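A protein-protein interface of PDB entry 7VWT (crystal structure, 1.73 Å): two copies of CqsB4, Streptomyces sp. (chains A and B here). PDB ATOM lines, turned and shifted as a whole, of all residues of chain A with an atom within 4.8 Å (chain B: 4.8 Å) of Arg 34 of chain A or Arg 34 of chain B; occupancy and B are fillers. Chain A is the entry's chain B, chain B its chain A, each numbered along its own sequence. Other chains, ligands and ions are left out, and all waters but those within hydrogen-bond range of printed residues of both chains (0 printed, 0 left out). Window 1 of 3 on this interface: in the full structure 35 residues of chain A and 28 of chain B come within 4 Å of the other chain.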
ATOM      1  N   LYS A  31       4.364  17.653 -19.500  1.00  0.00           N
ATOM      2  CA  LYS A  31       3.530  18.119 -18.397  1.00  0.00           C
ATOM      3  C   LYS A  31       2.189  18.655 -18.892  1.00  0.00           C
ATOM      4  O   LYS A  31       1.140  18.195 -18.450  1.00  0.00           O
ATOM      5  CB  LYS A  31       4.272  19.186 -17.592  1.00  0.00           C
ATOM      6  CG  LYS A  31       3.360  19.969 -16.637  1.00  0.00           C
ATOM      7  CD  LYS A  31       4.137  20.869 -15.722  1.00  0.00           C
ATOM      8  CE  LYS A  31       3.260  21.276 -14.566  1.00  0.00           C
ATOM      9  NZ  LYS A  31       4.046  21.493 -13.320  1.00  0.00           N
ATOM     10  N   ILE A  32       2.198  19.609 -19.832  1.00  0.00           N
ATOM     11  CA  ILE A  32       0.975  20.322 -20.204  1.00  0.00           C
ATOM     12  C   ILE A  32       0.276  19.736 -21.418  1.00  0.00           C
ATOM     13  O   ILE A  32      -0.854  20.157 -21.726  1.00  0.00           O
ATOM     14  CB  ILE A  32       1.243  21.820 -20.485  1.00  0.00           C
ATOM     15  CG1 ILE A  32       2.025  21.969 -21.789  1.00  0.00           C
ATOM     16  CG2 ILE A  32       1.958  22.444 -19.317  1.00  0.00           C
ATOM     17  CD1 ILE A  32       2.232  23.432 -22.254  1.00  0.00           C
ATOM     18  N   GLY A  33       0.911  18.803 -22.135  1.00  0.00           N
ATOM     19  CA  GLY A  33       0.401  18.425 -23.436  1.00  0.00           C
ATOM     20  C   GLY A  33      -0.993  17.842 -23.354  1.00  0.00           C
ATOM     21  O   GLY A  33      -1.825  18.077 -24.229  1.00  0.00           O
ATOM     22  N   ARG A  34      -1.268  17.087 -22.294  1.00  0.00           N
ATOM     23  CA  ARG A  34      -2.598  16.524 -22.054  1.00  0.00           C
ATOM     24  C   ARG A  34      -3.119  15.816 -23.299  1.00  0.00           C
ATOM     25  O   ARG A  34      -4.249  16.026 -23.747  1.00  0.00           O
ATOM     26  CB  ARG A  34      -3.567  17.606 -21.580  1.00  0.00           C
ATOM     27  CG  ARG A  34      -3.179  18.216 -20.229  1.00  0.00           C
ATOM     28  CD  ARG A  34      -3.986  19.491 -19.939  1.00  0.00           C
ATOM     29  NE  ARG A  34      -3.379  20.307 -18.882  1.00  0.00           N
ATOM     30  CZ  ARG A  34      -2.855  21.519 -19.066  1.00  0.00           C
ATOM     31  NH1 ARG A  34      -2.863  22.072 -20.273  1.00  0.00           N
ATOM     32  NH2 ARG A  34      -2.332  22.186 -18.037  1.00  0.00           N
ATOM     33  N   GLY A  35      -2.255  14.979 -23.877  1.00  0.00           N
ATOM     34  CA  GLY A  35      -2.643  14.127 -24.976  1.00  0.00           C
ATOM     35  C   GLY A  35      -2.648  14.788 -26.335  1.00  0.00           C
ATOM     36  O   GLY A  35      -2.917  14.106 -27.334  1.00  0.00           O
ATOM     37  N   ARG A  36      -2.392  16.091 -26.418  1.00  0.00           N
ATOM     38  CA  ARG A  36      -2.186  16.705 -27.723  1.00  0.00           C
ATOM     39  C   ARG A  36      -0.921  16.126 -28.351  1.00  0.00           C
ATOM     40  O   ARG A  36       0.020  15.756 -27.650  1.00  0.00           O
ATOM     41  CB  ARG A  36      -2.079  18.223 -27.579  1.00  0.00           C
ATOM     42  CG  ARG A  36      -3.365  18.835 -27.077  1.00  0.00           C
ATOM     43  CD  ARG A  36      -3.219  20.283 -26.695  1.00  0.00           C
ATOM     44  NE  ARG A  36      -2.505  20.465 -25.433  1.00  0.00           N
ATOM     45  CZ  ARG A  36      -2.321  21.656 -24.868  1.00  0.00           C
ATOM     46  NH1 ARG A  36      -1.676  21.765 -23.721  1.00  0.00           N
ATOM     47  NH2 ARG A  36      -2.801  22.738 -25.459  1.00  0.00           N
ATOM     48  N   ASP A  63      -2.588  27.297 -24.254  1.00  0.00           N
ATOM     49  CA  ASP A  63      -3.080  27.189 -22.876  1.00  0.00           C
ATOM     50  C   ASP A  63      -3.085  28.534 -22.162  1.00  0.00           C
ATOM     51  O   ASP A  63      -4.016  28.849 -21.413  1.00  0.00           O
ATOM     52  CB  ASP A  63      -2.220  26.201 -22.075  1.00  0.00           C
ATOM     53  CG  ASP A  63      -2.485  24.761 -22.460  1.00  0.00           C
ATOM     54  OD1 ASP A  63      -3.353  24.515 -23.345  1.00  0.00           O
ATOM     55  OD2 ASP A  63      -1.804  23.877 -21.896  1.00  0.00           O
ATOM     56  N   VAL A 295     -12.644  11.278 -24.200  1.00  0.00           N
ATOM     57  CA  VAL A 295     -11.388  11.846 -23.734  1.00  0.00           C
ATOM     58  C   VAL A 295     -10.399  11.823 -24.890  1.00  0.00           C
ATOM     59  O   VAL A 295     -10.030  10.748 -25.383  1.00  0.00           O
ATOM     60  CB  VAL A 295     -10.840  11.091 -22.517  1.00  0.00           C
ATOM     61  CG1 VAL A 295      -9.481  11.684 -22.106  1.00  0.00           C
ATOM     62  CG2 VAL A 295     -11.854  11.161 -21.375  1.00  0.00           C
ATOM     63  N   SER A 296      -9.971  13.012 -25.314  1.00  0.00           N
ATOM     64  CA  SER A 296      -9.081  13.164 -26.455  1.00  0.00           C
ATOM     65  C   SER A 296      -7.636  12.863 -26.073  1.00  0.00           C
ATOM     66  O   SER A 296      -7.191  13.142 -24.954  1.00  0.00           O
ATOM     67  CB  SER A 296      -9.167  14.587 -27.011  1.00  0.00           C
ATOM     68  OG  SER A 296      -8.696  15.528 -26.056  1.00  0.00           O
ATOM     69  N   GLY A 297      -6.903  12.297 -27.026  1.00  0.00           N
ATOM     70  CA  GLY A 297      -5.475  12.117 -26.854  1.00  0.00           C
ATOM     71  C   GLY A 297      -5.088  10.984 -25.935  1.00  0.00           C
ATOM     72  O   GLY A 297      -4.079  11.083 -25.221  1.00  0.00           O
ATOM     73  N   ARG A 298      -5.860   9.904 -25.930  1.00  0.00           N
ATOM     74  CA  ARG A 298      -5.542   8.741 -25.123  1.00  0.00           C
ATOM     75  C   ARG A 298      -4.834   7.687 -25.958  1.00  0.00           C
ATOM     76  O   ARG A 298      -4.958   7.632 -27.185  1.00  0.00           O
ATOM     77  CB  ARG A 298      -6.803   8.155 -24.481  1.00  0.00           C
ATOM     78  CG  ARG A 298      -7.412   9.097 -23.447  1.00  0.00           C
ATOM     79  CD  ARG A 298      -8.712   8.564 -22.884  1.00  0.00           C
ATOM     80  NE  ARG A 298      -9.591   8.075 -23.941  1.00  0.00           N
ATOM     81  CZ  ARG A 298      -9.656   6.806 -24.333  1.00  0.00           C
ATOM     82  NH1 ARG A 298     -10.485   6.469 -25.310  1.00  0.00           N
ATOM     83  NH2 ARG A 298      -8.902   5.883 -23.746  1.00  0.00           N
ATOM     84  N   PHE B  29     -14.554  17.616 -15.135  1.00  0.00           N
ATOM     85  CA  PHE B  29     -13.788  16.403 -14.839  1.00  0.00           C
ATOM     86  C   PHE B  29     -13.279  15.720 -16.117  1.00  0.00           C
ATOM     87  O   PHE B  29     -12.169  15.189 -16.147  1.00  0.00           O
ATOM     88  CB  PHE B  29     -14.692  15.462 -14.048  1.00  0.00           C
ATOM     89  CG  PHE B  29     -14.071  14.121 -13.646  1.00  0.00           C
ATOM     90  CD1 PHE B  29     -14.885  13.001 -13.581  1.00  0.00           C
ATOM     91  CD2 PHE B  29     -12.737  13.986 -13.294  1.00  0.00           C
ATOM     92  CE1 PHE B  29     -14.394  11.760 -13.173  1.00  0.00           C
ATOM     93  CE2 PHE B  29     -12.213  12.729 -12.914  1.00  0.00           C
ATOM     94  CZ  PHE B  29     -13.043  11.620 -12.837  1.00  0.00           C
ATOM     95  N   ARG B  30     -14.084  15.703 -17.179  1.00  0.00           N
ATOM     96  CA  ARG B  30     -13.611  15.139 -18.439  1.00  0.00           C
ATOM     97  C   ARG B  30     -12.355  15.857 -18.918  1.00  0.00           C
ATOM     98  O   ARG B  30     -11.385  15.225 -19.347  1.00  0.00           O
ATOM     99  CB  ARG B  30     -14.704  15.253 -19.502  1.00  0.00           C
ATOM    100  CG  ARG B  30     -14.403  14.441 -20.771  1.00  0.00           C
ATOM    101  CD  ARG B  30     -15.572  14.475 -21.756  1.00  0.00           C
ATOM    102  NE  ARG B  30     -15.925  15.842 -22.116  1.00  0.00           N
ATOM    103  CZ  ARG B  30     -15.395  16.524 -23.134  1.00  0.00           C
ATOM    104  NH1 ARG B  30     -15.785  17.791 -23.360  1.00  0.00           N
ATOM    105  NH2 ARG B  30     -14.489  15.962 -23.932  1.00  0.00           N
ATOM    106  N   LYS B  31     -12.400  17.187 -18.865  1.00  0.00           N
ATOM    107  CA  LYS B  31     -11.360  18.095 -19.353  1.00  0.00           C
ATOM    108  C   LYS B  31     -10.099  18.048 -18.502  1.00  0.00           C
ATOM    109  O   LYS B  31      -8.982  18.017 -19.042  1.00  0.00           O
ATOM    110  CB  LYS B  31     -11.920  19.516 -19.353  1.00  0.00           C
ATOM    111  CG  LYS B  31     -10.949  20.616 -19.808  1.00  0.00           C
ATOM    112  CD  LYS B  31     -11.573  21.994 -19.664  1.00  0.00           C
ATOM    113  CE  LYS B  31     -10.996  23.004 -20.657  1.00  0.00           C
ATOM    114  NZ  LYS B  31      -9.558  23.295 -20.392  1.00  0.00           N
ATOM    115  N   ILE B  32     -10.250  18.063 -17.174  1.00  0.00           N
ATOM    116  CA  ILE B  32      -9.099  18.096 -16.267  1.00  0.00           C
ATOM    117  C   ILE B  32      -8.683  16.698 -15.823  1.00  0.00           C
ATOM    118  O   ILE B  32      -7.487  16.393 -15.738  1.00  0.00           O
ATOM    119  CB  ILE B  32      -9.412  18.992 -15.056  1.00  0.00           C
ATOM    120  CG1 ILE B  32      -9.629  20.427 -15.509  1.00  0.00           C
ATOM    121  CG2 ILE B  32      -8.266  18.957 -14.059  1.00  0.00           C
ATOM    122  CD1 ILE B  32     -10.247  21.242 -14.470  1.00  0.00           C
ATOM    123  N   GLY B  33      -9.654  15.839 -15.517  1.00  0.00           N
ATOM    124  CA  GLY B  33      -9.330  14.493 -15.089  1.00  0.00           C
ATOM    125  C   GLY B  33      -8.863  13.612 -16.226  1.00  0.00           C
ATOM    126  O   GLY B  33      -8.077  12.689 -16.004  1.00  0.00           O
ATOM    127  N   ARG B  34      -9.319  13.898 -17.460  1.00  0.00           N
ATOM    128  CA  ARG B  34      -8.910  13.155 -18.653  1.00  0.00           C
ATOM    129  C   ARG B  34      -9.069  11.644 -18.468  1.00  0.00           C
ATOM    130  O   ARG B  34     -10.192  11.153 -18.381  1.00  0.00           O
ATOM    131  CB  ARG B  34      -7.472  13.520 -19.030  1.00  0.00           C
ATOM    132  CG  ARG B  34      -7.313  15.027 -19.360  1.00  0.00           C
ATOM    133  CD  ARG B  34      -5.995  15.328 -20.049  1.00  0.00           C
ATOM    134  NE  ARG B  34      -5.614  14.234 -20.934  1.00  0.00           N
ATOM    135  CZ  ARG B  34      -6.145  14.011 -22.134  1.00  0.00           C
ATOM    136  NH1 ARG B  34      -5.722  12.978 -22.853  1.00  0.00           N
ATOM    137  NH2 ARG B  34      -7.085  14.820 -22.621  1.00  0.00           N
ATOM    138  N   GLY B  35      -7.965  10.899 -18.399  1.00  0.00           N
ATOM    139  CA  GLY B  35      -8.075   9.445 -18.314  1.00  0.00           C
ATOM    140  C   GLY B  35      -8.837   8.977 -17.085  1.00  0.00           C
ATOM    141  O   GLY B  35      -9.561   7.973 -17.134  1.00  0.00           O
ATOM    142  N   ARG B  36      -8.693   9.700 -15.968  1.00  0.00           N
ATOM    143  CA  ARG B  36      -9.423   9.357 -14.751  1.00  0.00           C
ATOM    144  C   ARG B  36     -10.931   9.425 -14.958  1.00  0.00           C
ATOM    145  O   ARG B  36     -11.671   8.719 -14.278  1.00  0.00           O
ATOM    146  CB  ARG B  36      -9.025  10.285 -13.596  1.00  0.00           C
ATOM    147  CG  ARG B  36      -7.545  10.181 -13.193  1.00  0.00           C
ATOM    148  CD  ARG B  36      -7.072  11.367 -12.318  1.00  0.00           C
ATOM    149  NE  ARG B  36      -6.869  12.621 -13.055  1.00  0.00           N
ATOM    150  CZ  ARG B  36      -6.421  13.755 -12.499  1.00  0.00           C
ATOM    151  NH1 ARG B  36      -6.280  14.858 -13.226  1.00  0.00           N
ATOM    152  NH2 ARG B  36      -6.105  13.788 -11.208  1.00  0.00           N
ATOM    153  N   PHE B  37     -11.407  10.277 -15.873  1.00  0.00           N
ATOM    154  CA  PHE B  37     -12.846  10.379 -16.150  1.00  0.00           C
ATOM    155  C   PHE B  37     -13.430   9.046 -16.622  1.00  0.00           C
ATOM    156  O   PHE B  37     -14.584   8.734 -16.317  1.00  0.00           O
ATOM    157  CB  PHE B  37     -13.061  11.488 -17.198  1.00  0.00           C
ATOM    158  CG  PHE B  37     -14.484  11.617 -17.736  1.00  0.00           C
ATOM    159  CD1 PHE B  37     -15.425  12.385 -17.069  1.00  0.00           C
ATOM    160  CD2 PHE B  37     -14.831  11.058 -18.954  1.00  0.00           C
ATOM    161  CE1 PHE B  37     -16.700  12.553 -17.571  1.00  0.00           C
ATOM    162  CE2 PHE B  37     -16.109  11.234 -19.471  1.00  0.00           C
ATOM    163  CZ  PHE B  37     -17.035  11.972 -18.782  1.00  0.00           C
ATOM    164  N   LEU B  38     -12.643   8.239 -17.342  1.00  0.00           N
ATOM    165  CA  LEU B  38     -13.142   6.989 -17.895  1.00  0.00           C
ATOM    166  C   LEU B  38     -13.442   5.975 -16.801  1.00  0.00           C
ATOM    167  O   LEU B  38     -14.242   5.069 -17.025  1.00  0.00           O
ATOM    168  CB  LEU B  38     -12.144   6.406 -18.899  1.00  0.00           C
ATOM    169  CG  LEU B  38     -12.022   7.139 -20.234  1.00  0.00           C
ATOM    170  CD1 LEU B  38     -11.089   6.400 -21.154  1.00  0.00           C
ATOM    171  CD2 LEU B  38     -13.393   7.296 -20.856  1.00  0.00           C
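O of Arg 34 of chain A sits close to NH2 of Arg 34 of chain B (3.3 Å). The guanidinium group (NH1) of Arg 34 of chain B sits at hydrogen-bond distance from the backbone carbonyl oxygen (O) of Ser 296 of chain A (2.6 Å). NH1 of Arg 34 of chain B sits at hydrogen-bond distance from O of Gly 297 of chain A (3.4 Å).
The backbone carbonyl oxygen of Phe 29 of chain B is in hydrogen-bond range of the backbone NH of Arg 34 of chain B (3.4 Å). The backbone carbonyl oxygen (O) of Ile 32 of chain A sits at hydrogen-bond distance from the guanidinium group (NH1) of Arg 34 of chain A (3.1 Å). The side-chain carboxylate (OD2) of Asp 63 of chain A lies within salt-bridge range of the guanidinium group (NH1) of Arg 34 of chain A (2.6 Å). The backbone carbonyl oxygen of Val 295 of chain A is in hydrogen-bond range of the guanidinium group of Arg 298 of chain A, at 3.1 Å.
Among the printed residues, pairs that only touch across the chains: Gly 35 of chain A with Arg 34 of chain B, Val 295 of chain A with Arg 34 of chain B, Val 295 of chain A with Phe 37 of chain B and Arg 298 of chain A with Leu 38 of chain B.
Arg 34 of chain A touches just one residue of chain B: Arg 34 (3.2 Å). Of chain A, only Arg 34 (3.2 Å), Gly 35 (3.9 Å), Val 295 (3.4 Å), Ser 296 (2.6 Å) and Gly 297 (3.4 Å) come within 4 Å of Arg 34 of chain B. Of the printed residues of chain B, Arg 298 of chain A touches Leu 38. Of the printed residues of chain B, Ser 296 of chain A touches Arg 34 (2.6 Å). Printed residues of chain A within 4 Å of Leu 38 of chain B: Arg 298. Printed residues of chain B within 4 Å of Val 295 of chain A: Arg 34 and Phe 37. Arg 30 of chain B touches none of the printed residues of chain A. The nearest printed residue of chain B that does not touch Arg 34 of chain A is Lys 31 of chain B (5.3 Å). The nearest residue of chain A that does not touch Arg 34 of chain B is Arg 298 of chain A (4.3 Å). The nearest printed residue of chain B that does not touch Gly 297 of chain A is Gly 35 of chain B (7.9 Å).
Printed residues of chain A that touch a printed residue of chain B: Arg 34, Gly 35, Val 295, Ser 296, Gly 297 and Arg 298. Hydrophobic or aromatic side chains of chain A within 4 Å of the printed part of chain B: Val 295. Among the printed residues, 7 pairs touch across the chains. Among the printed residues, no Asp or Glu carboxylate lies within 4 Å of a Lys or Arg side-chain nitrogen of the other chain.
Arg 34 of chain B touches its own counterpart, Arg 34 of chain A. Gly 35 of chain A touches Arg 34 of chain B, but with the chains exchanged Arg 34 of chain A does not touch Gly 35 of chain B (8.3 Å). Positions printed for both chains: 31, 32, 33, 34, 35 and 36. Of the 7 pairs that touch across the chains among the printed residues, 1 has its exchanged pair printed and touching as well.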
